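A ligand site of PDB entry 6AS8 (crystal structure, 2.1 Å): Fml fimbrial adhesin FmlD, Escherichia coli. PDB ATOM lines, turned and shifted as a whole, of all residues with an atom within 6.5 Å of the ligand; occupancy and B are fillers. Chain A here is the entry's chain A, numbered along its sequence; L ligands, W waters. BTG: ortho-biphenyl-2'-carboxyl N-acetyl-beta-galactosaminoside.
The backbone NH (N) of Thr 135 lies within hydrogen-bond range of the side-chain carboxylate (OD1) of Asp 51 (3.0 Å). The side-chain carboxylate (OD1) of Asp 45 is in hydrogen-bond range of the indole nitrogen (NE1) of Trp 43, 3.2 Å away. N of Leu 136 lies within hydrogen-bond range of OD1 of Asp 51. The side-chain carboxylate of Asp 45 is in hydrogen-bond range of the backbone NH of Phe 1 (2.8 Å). OG of Ser 2 sits at hydrogen-bond distance from OD2 of Asp 45 (2.7 Å). The backbone carbonyl oxygen of Asn 140 is in hydrogen-bond range of the side-chain amino group of Lys 132. O of Ser 2 sits at hydrogen-bond distance from N of Trp 43 (2.9 Å). The side-chain amino group (NZ) of Lys 132 lies within hydrogen-bond range of the backbone carbonyl oxygen (O) of Gly 139, 3.3 Å away.
Water W2 lies within hydrogen-bond range of the side-chain amino group (NZ) of Lys 132 (2.6 Å), an oxygen (O7) of the ligand (2.7 Å) and the backbone NH (N) of Phe 1 (3.1 Å). Water W1 lies within hydrogen-bond range of the backbone carbonyl oxygen (O) of Leu 136 (2.6 Å), the side-chain carboxylate (OD2) of Asp 51 (2.7 Å), an oxygen (O3) of the ligand (3.1 Å) and the side-chain amide nitrogen (ND2) of Asn 140 (3.4 Å).
The guanidinium group (NE) of Arg 142 is in salt-bridge range of an oxygen (O23) of the ligand. The backbone carbonyl oxygen (O) of Gly 139 sits at hydrogen-bond distance from an oxygen (O3) of the ligand (3.4 Å). The backbone NH (N) of Phe 1 lies within hydrogen-bond range of an oxygen (O6) of the ligand. The side-chain amino group (NZ) of Lys 132 sits at hydrogen-bond distance from an oxygen (O3) of the ligand. OD1 of Asn 44 lies close to O6 of the ligand (3.5 Å). OD1 of Asp 53 sits at hydrogen-bond distance from O4 of the ligand, 2.4 Å away. O6 of the ligand lies within hydrogen-bond range of N of Asp 45 (3.0 Å). An oxygen (O3) of the ligand is in hydrogen-bond range of the side-chain amide nitrogen (ND2) of Asn 140 (3.1 Å).
Ser 2 touches the ligand (OG to C18, 3.6 Å). CA of Gly 12 touches C19 of the ligand (3.7 Å). Tyr 46 touches the ligand (CE1 to C13, 3.4 Å). OD2 of Asp 51 touches C4 of the ligand, 3.3 Å away. Ala 134 touches the ligand (CB to O3, 3.3 Å). Within 4 Å of the ligand: Phe 1, Ser 2, Gly 12, Asn 44, Asp 45, Tyr 46, Asp 51, Asp 53, Lys 132, Ala 134, Gly 139, Asn 140 and Arg 142. The nearest printed residue that does not touch the ligand is Trp 43 (4.7 Å).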
ATOM      1  N   PHE A   1      11.846  -6.148   1.074  1.00  0.00           N
ATOM      2  CA  PHE A   1      13.080  -5.383   1.429  1.00  0.00           C
ATOM      3  C   PHE A   1      13.243  -4.183   0.504  1.00  0.00           C
ATOM      4  O   PHE A   1      13.094  -4.300  -0.706  1.00  0.00           O
ATOM      5  CB  PHE A   1      14.306  -6.274   1.348  1.00  0.00           C
ATOM      6  CG  PHE A   1      15.585  -5.561   1.674  1.00  0.00           C
ATOM      7  CD1 PHE A   1      16.423  -5.108   0.660  1.00  0.00           C
ATOM      8  CD2 PHE A   1      15.966  -5.337   2.994  1.00  0.00           C
ATOM      9  CE1 PHE A   1      17.601  -4.458   0.950  1.00  0.00           C
ATOM     10  CE2 PHE A   1      17.140  -4.680   3.290  1.00  0.00           C
ATOM     11  CZ  PHE A   1      17.966  -4.244   2.269  1.00  0.00           C
ATOM     12  N   SER A   2      13.552  -3.028   1.088  1.00  0.00           N
ATOM     13  CA  SER A   2      13.710  -1.799   0.319  1.00  0.00           C
ATOM     14  C   SER A   2      14.789  -0.898   0.901  1.00  0.00           C
ATOM     15  O   SER A   2      15.149  -1.031   2.079  1.00  0.00           O
ATOM     16  CB  SER A   2      12.382  -1.050   0.239  1.00  0.00           C
ATOM     17  OG  SER A   2      11.389  -1.837  -0.369  1.00  0.00           O
ATOM     18  N   ILE A  11      13.685   1.769  -3.135  1.00  0.00           N
ATOM     19  CA  ILE A  11      14.439   1.012  -4.126  1.00  0.00           C
ATOM     20  C   ILE A  11      14.361  -0.477  -3.792  1.00  0.00           C
ATOM     21  O   ILE A  11      14.714  -0.884  -2.689  1.00  0.00           O
ATOM     22  CB  ILE A  11      15.907   1.453  -4.183  1.00  0.00           C
ATOM     23  CG1 ILE A  11      16.006   2.968  -4.374  1.00  0.00           C
ATOM     24  CG2 ILE A  11      16.643   0.722  -5.305  1.00  0.00           C
ATOM     25  CD1 ILE A  11      17.385   3.539  -4.090  1.00  0.00           C
ATOM     26  N   GLY A  12      13.874  -1.270  -4.743  1.00  0.00           N
ATOM     27  CA  GLY A  12      13.700  -2.704  -4.528  1.00  0.00           C
ATOM     28  C   GLY A  12      14.850  -3.507  -5.102  1.00  0.00           C
ATOM     29  O   GLY A  12      15.099  -4.637  -4.675  1.00  0.00           O
ATOM     30  N   ALA A  13      15.550  -2.925  -6.070  1.00  0.00           N
ATOM     31  CA  ALA A  13      16.673  -3.578  -6.718  1.00  0.00           C
ATOM     32  C   ALA A  13      17.354  -2.613  -7.690  1.00  0.00           C
ATOM     33  O   ALA A  13      16.871  -1.490  -7.876  1.00  0.00           O
ATOM     34  CB  ALA A  13      16.228  -4.837  -7.460  1.00  0.00           C
ATOM     35  N   TRP A  43      15.346  -1.113   4.994  1.00  0.00           N
ATOM     36  CA  TRP A  43      14.372  -1.590   5.989  1.00  0.00           C
ATOM     37  C   TRP A  43      13.626  -2.827   5.523  1.00  0.00           C
ATOM     38  O   TRP A  43      13.614  -3.157   4.334  1.00  0.00           O
ATOM     39  CB  TRP A  43      13.370  -0.478   6.308  1.00  0.00           C
ATOM     40  CG  TRP A  43      12.584  -0.021   5.119  1.00  0.00           C
ATOM     41  CD1 TRP A  43      11.370  -0.499   4.698  1.00  0.00           C
ATOM     42  CD2 TRP A  43      12.960   1.000   4.187  1.00  0.00           C
ATOM     43  NE1 TRP A  43      10.970   0.166   3.558  1.00  0.00           N
ATOM     44  CE2 TRP A  43      11.922   1.091   3.225  1.00  0.00           C
ATOM     45  CE3 TRP A  43      14.063   1.845   4.064  1.00  0.00           C
ATOM     46  CZ2 TRP A  43      11.965   2.001   2.166  1.00  0.00           C
ATOM     47  CZ3 TRP A  43      14.100   2.744   3.012  1.00  0.00           C
ATOM     48  CH2 TRP A  43      13.065   2.807   2.080  1.00  0.00           C
ATOM     49  N   ASN A  44      12.991  -3.495   6.479  1.00  0.00           N
ATOM     50  CA  ASN A  44      12.104  -4.616   6.194  1.00  0.00           C
ATOM     51  C   ASN A  44      10.709  -4.097   5.862  1.00  0.00           C
ATOM     52  O   ASN A  44      10.161  -3.262   6.571  1.00  0.00           O
ATOM     53  CB  ASN A  44      12.041  -5.566   7.388  1.00  0.00           C
ATOM     54  CG  ASN A  44      11.338  -6.870   7.064  1.00  0.00           C
ATOM     55  OD1 ASN A  44      10.114  -6.920   6.957  1.00  0.00           O
ATOM     56  ND2 ASN A  44      12.115  -7.941   6.928  1.00  0.00           N
ATOM     57  N   ASP A  45      10.136  -4.593   4.763  1.00  0.00           N
ATOM     58  CA  ASP A  45       8.870  -4.056   4.250  1.00  0.00           C
ATOM     59  C   ASP A  45       7.646  -4.556   5.009  1.00  0.00           C
ATOM     60  O   ASP A  45       6.544  -4.020   4.839  1.00  0.00           O
ATOM     61  CB  ASP A  45       8.732  -4.375   2.765  1.00  0.00           C
ATOM     62  CG  ASP A  45       9.495  -3.401   1.886  1.00  0.00           C
ATOM     63  OD1 ASP A  45       9.337  -2.182   2.068  1.00  0.00           O
ATOM     64  OD2 ASP A  45      10.252  -3.864   1.010  1.00  0.00           O
ATOM     65  N   TYR A  46       7.822  -5.590   5.837  1.00  0.00           N
ATOM     66  CA  TYR A  46       6.741  -6.087   6.687  1.00  0.00           C
ATOM     67  C   TYR A  46       6.945  -5.618   8.130  1.00  0.00           C
ATOM     68  O   TYR A  46       6.009  -5.183   8.790  1.00  0.00           O
ATOM     69  CB  TYR A  46       6.651  -7.611   6.644  1.00  0.00           C
ATOM     70  CG  TYR A  46       6.250  -8.171   5.301  1.00  0.00           C
ATOM     71  CD1 TYR A  46       5.322  -7.521   4.496  1.00  0.00           C
ATOM     72  CD2 TYR A  46       6.796  -9.361   4.835  1.00  0.00           C
ATOM     73  CE1 TYR A  46       4.946  -8.037   3.266  1.00  0.00           C
ATOM     74  CE2 TYR A  46       6.422  -9.884   3.613  1.00  0.00           C
ATOM     75  CZ  TYR A  46       5.506  -9.217   2.830  1.00  0.00           C
ATOM     76  OH  TYR A  46       5.141  -9.734   1.608  1.00  0.00           O
ATOM     77  N   GLY A  47       8.182  -5.714   8.607  1.00  0.00           N
ATOM     78  CA  GLY A  47       8.497  -5.384   9.980  1.00  0.00           C
ATOM     79  C   GLY A  47       8.168  -6.542  10.908  1.00  0.00           C
ATOM     80  O   GLY A  47       7.719  -7.594  10.456  1.00  0.00           O
ATOM     81  N   ASP A  51       9.458 -11.905   8.224  1.00  0.00           N
ATOM     82  CA  ASP A  51      10.264 -12.403   7.120  1.00  0.00           C
ATOM     83  C   ASP A  51      11.571 -11.614   7.047  1.00  0.00           C
ATOM     84  O   ASP A  51      11.701 -10.684   6.245  1.00  0.00           O
ATOM     85  CB  ASP A  51       9.488 -12.299   5.805  1.00  0.00           C
ATOM     86  CG  ASP A  51      10.218 -12.956   4.637  1.00  0.00           C
ATOM     87  OD1 ASP A  51      11.170 -13.720   4.888  1.00  0.00           O
ATOM     88  OD2 ASP A  51       9.815 -12.715   3.480  1.00  0.00           O
ATOM     89  N   THR A  52      12.520 -11.992   7.892  1.00  0.00           N
ATOM     90  CA  THR A  52      13.760 -11.235   8.056  1.00  0.00           C
ATOM     91  C   THR A  52      14.613 -11.226   6.793  1.00  0.00           C
ATOM     92  O   THR A  52      14.757 -12.247   6.111  1.00  0.00           O
ATOM     93  CB  THR A  52      14.602 -11.801   9.219  1.00  0.00           C
ATOM     94  OG1 THR A  52      13.819 -11.782  10.424  1.00  0.00           O
ATOM     95  CG2 THR A  52      15.871 -10.981   9.432  1.00  0.00           C
ATOM     96  N   ASP A  53      15.185 -10.060   6.498  1.00  0.00           N
ATOM     97  CA  ASP A  53      16.053  -9.893   5.337  1.00  0.00           C
ATOM     98  C   ASP A  53      17.507 -10.067   5.724  1.00  0.00           C
ATOM     99  O   ASP A  53      17.907  -9.713   6.834  1.00  0.00           O
ATOM    100  CB  ASP A  53      15.847  -8.501   4.724  1.00  0.00           C
ATOM    101  CG  ASP A  53      14.436  -8.306   4.206  1.00  0.00           C
ATOM    102  OD1 ASP A  53      13.976  -9.165   3.431  1.00  0.00           O
ATOM    103  OD2 ASP A  53      13.790  -7.307   4.578  1.00  0.00           O
ATOM    104  N   ILE A  94      18.035  -7.481   8.642  1.00  0.00           N
ATOM    105  CA  ILE A  94      17.056  -6.396   8.709  1.00  0.00           C
ATOM    106  C   ILE A  94      15.648  -6.971   8.891  1.00  0.00           C
ATOM    107  O   ILE A  94      15.213  -7.815   8.119  1.00  0.00           O
ATOM    108  CB  ILE A  94      17.084  -5.534   7.424  1.00  0.00           C
ATOM    109  CG1 ILE A  94      18.505  -5.009   7.159  1.00  0.00           C
ATOM    110  CG2 ILE A  94      16.088  -4.383   7.507  1.00  0.00           C
ATOM    111  CD1 ILE A  94      19.054  -4.100   8.239  1.00  0.00           C
ATOM    112  N   LYS A 132      20.715  -9.261  -1.379  1.00  0.00           N
ATOM    113  CA  LYS A 132      19.652  -9.470  -0.397  1.00  0.00           C
ATOM    114  C   LYS A 132      18.992 -10.826  -0.580  1.00  0.00           C
ATOM    115  O   LYS A 132      18.801 -11.273  -1.709  1.00  0.00           O
ATOM    116  CB  LYS A 132      18.596  -8.357  -0.502  1.00  0.00           C
ATOM    117  CG  LYS A 132      17.309  -8.636   0.276  1.00  0.00           C
ATOM    118  CD  LYS A 132      16.216  -9.244  -0.591  1.00  0.00           C
ATOM    119  CE  LYS A 132      14.997  -9.644   0.228  1.00  0.00           C
ATOM    120  NZ  LYS A 132      13.838 -10.026  -0.626  1.00  0.00           N
ATOM    121  N   ILE A 133      18.656 -11.467   0.532  1.00  0.00           N
ATOM    122  CA  ILE A 133      17.801 -12.650   0.516  1.00  0.00           C
ATOM    123  C   ILE A 133      17.055 -12.728   1.842  1.00  0.00           C
ATOM    124  O   ILE A 133      17.622 -12.453   2.907  1.00  0.00           O
ATOM    125  CB  ILE A 133      18.593 -13.946   0.255  1.00  0.00           C
ATOM    126  CG1 ILE A 133      17.644 -15.137   0.138  1.00  0.00           C
ATOM    127  CG2 ILE A 133      19.608 -14.193   1.371  1.00  0.00           C
ATOM    128  CD1 ILE A 133      18.211 -16.284  -0.684  1.00  0.00           C
ATOM    129  N   ALA A 134      15.777 -13.102   1.786  1.00  0.00           N
ATOM    130  CA  ALA A 134      14.931 -13.131   2.966  1.00  0.00           C
ATOM    131  C   ALA A 134      14.924 -14.522   3.607  1.00  0.00           C
ATOM    132  O   ALA A 134      15.828 -15.323   3.365  1.00  0.00           O
ATOM    133  CB  ALA A 134      13.510 -12.704   2.599  1.00  0.00           C
ATOM    134  N   THR A 135      13.909 -14.793   4.433  1.00  0.00           N
ATOM    135  CA  THR A 135      13.847 -16.030   5.212  1.00  0.00           C
ATOM    136  C   THR A 135      12.772 -16.981   4.681  1.00  0.00           C
ATOM    137  O   THR A 135      12.983 -18.184   4.596  1.00  0.00           O
ATOM    138  CB  THR A 135      13.557 -15.717   6.699  1.00  0.00           C
ATOM    139  OG1 THR A 135      14.548 -14.817   7.210  1.00  0.00           O
ATOM    140  CG2 THR A 135      13.549 -16.991   7.535  1.00  0.00           C
ATOM    141  N   LEU A 136      11.611 -16.424   4.327  1.00  0.00           N
ATOM    142  CA  LEU A 136      10.474 -17.227   3.920  1.00  0.00           C
ATOM    143  C   LEU A 136      10.549 -17.632   2.458  1.00  0.00           C
ATOM    144  O   LEU A 136      10.935 -16.830   1.593  1.00  0.00           O
ATOM    145  CB  LEU A 136       9.170 -16.463   4.183  1.00  0.00           C
ATOM    146  CG  LEU A 136       8.434 -16.769   5.491  1.00  0.00           C
ATOM    147  CD1 LEU A 136       9.378 -16.827   6.685  1.00  0.00           C
ATOM    148  CD2 LEU A 136       7.340 -15.727   5.727  1.00  0.00           C
ATOM    149  N   GLY A 139      13.076 -16.753  -0.503  1.00  0.00           N
ATOM    150  CA  GLY A 139      13.774 -15.602   0.047  1.00  0.00           C
ATOM    151  C   GLY A 139      13.790 -14.425  -0.905  1.00  0.00           C
ATOM    152  O   GLY A 139      14.176 -13.319  -0.517  1.00  0.00           O
ATOM    153  N   ASN A 140      13.362 -14.660  -2.137  1.00  0.00           N
ATOM    154  CA  ASN A 140      13.272 -13.610  -3.157  1.00  0.00           C
ATOM    155  C   ASN A 140      14.543 -12.796  -3.263  1.00  0.00           C
ATOM    156  O   ASN A 140      14.558 -11.609  -2.936  1.00  0.00           O
ATOM    157  CB  ASN A 140      12.092 -12.686  -2.846  1.00  0.00           C
ATOM    158  CG  ASN A 140      10.780 -13.429  -2.775  1.00  0.00           C
ATOM    159  OD1 ASN A 140      10.432 -14.186  -3.686  1.00  0.00           O
ATOM    160  ND2 ASN A 140      10.043 -13.239  -1.694  1.00  0.00           N
ATOM    161  N   PRO A 141      15.635 -13.439  -3.708  1.00  0.00           N
ATOM    162  CA  PRO A 141      16.925 -12.736  -3.801  1.00  0.00           C
ATOM    163  C   PRO A 141      16.889 -11.531  -4.737  1.00  0.00           C
ATOM    164  O   PRO A 141      16.233 -11.583  -5.771  1.00  0.00           O
ATOM    165  CB  PRO A 141      17.875 -13.816  -4.312  1.00  0.00           C
ATOM    166  CG  PRO A 141      17.005 -14.845  -4.940  1.00  0.00           C
ATOM    167  CD  PRO A 141      15.743 -14.837  -4.150  1.00  0.00           C
ATOM    168  N   ARG A 142      17.593 -10.468  -4.360  1.00  0.00           N
ATOM    169  CA  ARG A 142      17.668  -9.268  -5.187  1.00  0.00           C
ATOM    170  C   ARG A 142      19.075  -8.697  -5.149  1.00  0.00           C
ATOM    171  O   ARG A 142      19.769  -8.805  -4.133  1.00  0.00           O
ATOM    172  CB  ARG A 142      16.667  -8.214  -4.715  1.00  0.00           C
ATOM    173  CG  ARG A 142      15.219  -8.664  -4.698  1.00  0.00           C
ATOM    174  CD  ARG A 142      14.650  -8.777  -6.112  1.00  0.00           C
ATOM    175  NE  ARG A 142      13.253  -9.196  -6.091  1.00  0.00           N
ATOM    176  CZ  ARG A 142      12.832 -10.461  -6.113  1.00  0.00           C
ATOM    177  NH1 ARG A 142      13.710 -11.456  -6.165  1.00  0.00           N
ATOM    178  NH2 ARG A 142      11.538 -10.720  -6.089  1.00  0.00           N
HETATM  179  C13 BTG L   1       5.928  -5.888   0.872  1.00  0.00           C
HETATM  180  C15 BTG L   1       6.737  -4.788  -1.096  1.00  0.00           C
HETATM  181  C17 BTG L   1       8.862  -5.557  -2.227  1.00  0.00           C
HETATM  182  C20 BTG L   1      10.781  -5.412  -4.227  1.00  0.00           C
HETATM  183  C21 BTG L   1       9.762  -6.352  -4.311  1.00  0.00           C
HETATM  184  C22 BTG L   1       9.704  -7.310  -5.485  1.00  0.00           C
HETATM  185  C2  BTG L   1      10.103  -9.568  -0.019  1.00  0.00           C
HETATM  186  C7  BTG L   1       9.791  -9.837  -2.461  1.00  0.00           C
HETATM  187  O3  BTG L   1      11.444 -11.489   0.390  1.00  0.00           O
HETATM  188  C3  BTG L   1      10.502 -10.626   0.982  1.00  0.00           C
HETATM  189  C4  BTG L   1      11.112  -9.950   2.176  1.00  0.00           C
HETATM  190  O4  BTG L   1      12.224  -9.185   1.766  1.00  0.00           O
HETATM  191  C5  BTG L   1      10.065  -9.050   2.785  1.00  0.00           C
HETATM  192  C6  BTG L   1      10.633  -8.363   4.004  1.00  0.00           C
HETATM  193  O6  BTG L   1      11.186  -7.117   3.634  1.00  0.00           O
HETATM  194  O5  BTG L   1       9.683  -8.084   1.826  1.00  0.00           O
HETATM  195  C1  BTG L   1       9.166  -8.560   0.603  1.00  0.00           C
HETATM  196  O1  BTG L   1       9.075  -7.501  -0.318  1.00  0.00           O
HETATM  197  C11 BTG L   1       7.952  -6.652  -0.190  1.00  0.00           C
HETATM  198  C12 BTG L   1       6.999  -6.777   0.826  1.00  0.00           C
HETATM  199  C14 BTG L   1       5.799  -4.897  -0.086  1.00  0.00           C
HETATM  200  C16 BTG L   1       7.810  -5.660  -1.142  1.00  0.00           C
HETATM  201  C18 BTG L   1       9.870  -4.616  -2.150  1.00  0.00           C
HETATM  202  C19 BTG L   1      10.829  -4.543  -3.143  1.00  0.00           C
HETATM  203  O23 BTG L   1      10.728  -7.950  -5.822  1.00  0.00           O
HETATM  204  O24 BTG L   1       8.628  -7.448  -6.121  1.00  0.00           O
HETATM  205  C25 BTG L   1       8.806  -6.431  -3.311  1.00  0.00           C
HETATM  206  N2  BTG L   1       9.444 -10.174  -1.129  1.00  0.00           N
HETATM  207  C8  BTG L   1       9.085 -10.493  -3.630  1.00  0.00           C
HETATM  208  O7  BTG L   1      10.662  -9.023  -2.690  1.00  0.00           O
HETATM  209  O   HOH W   1      10.653 -14.291   1.444  1.00  0.00           O
HETATM  210  O   HOH W   2      12.634  -7.827  -1.374  1.00  0.00           O
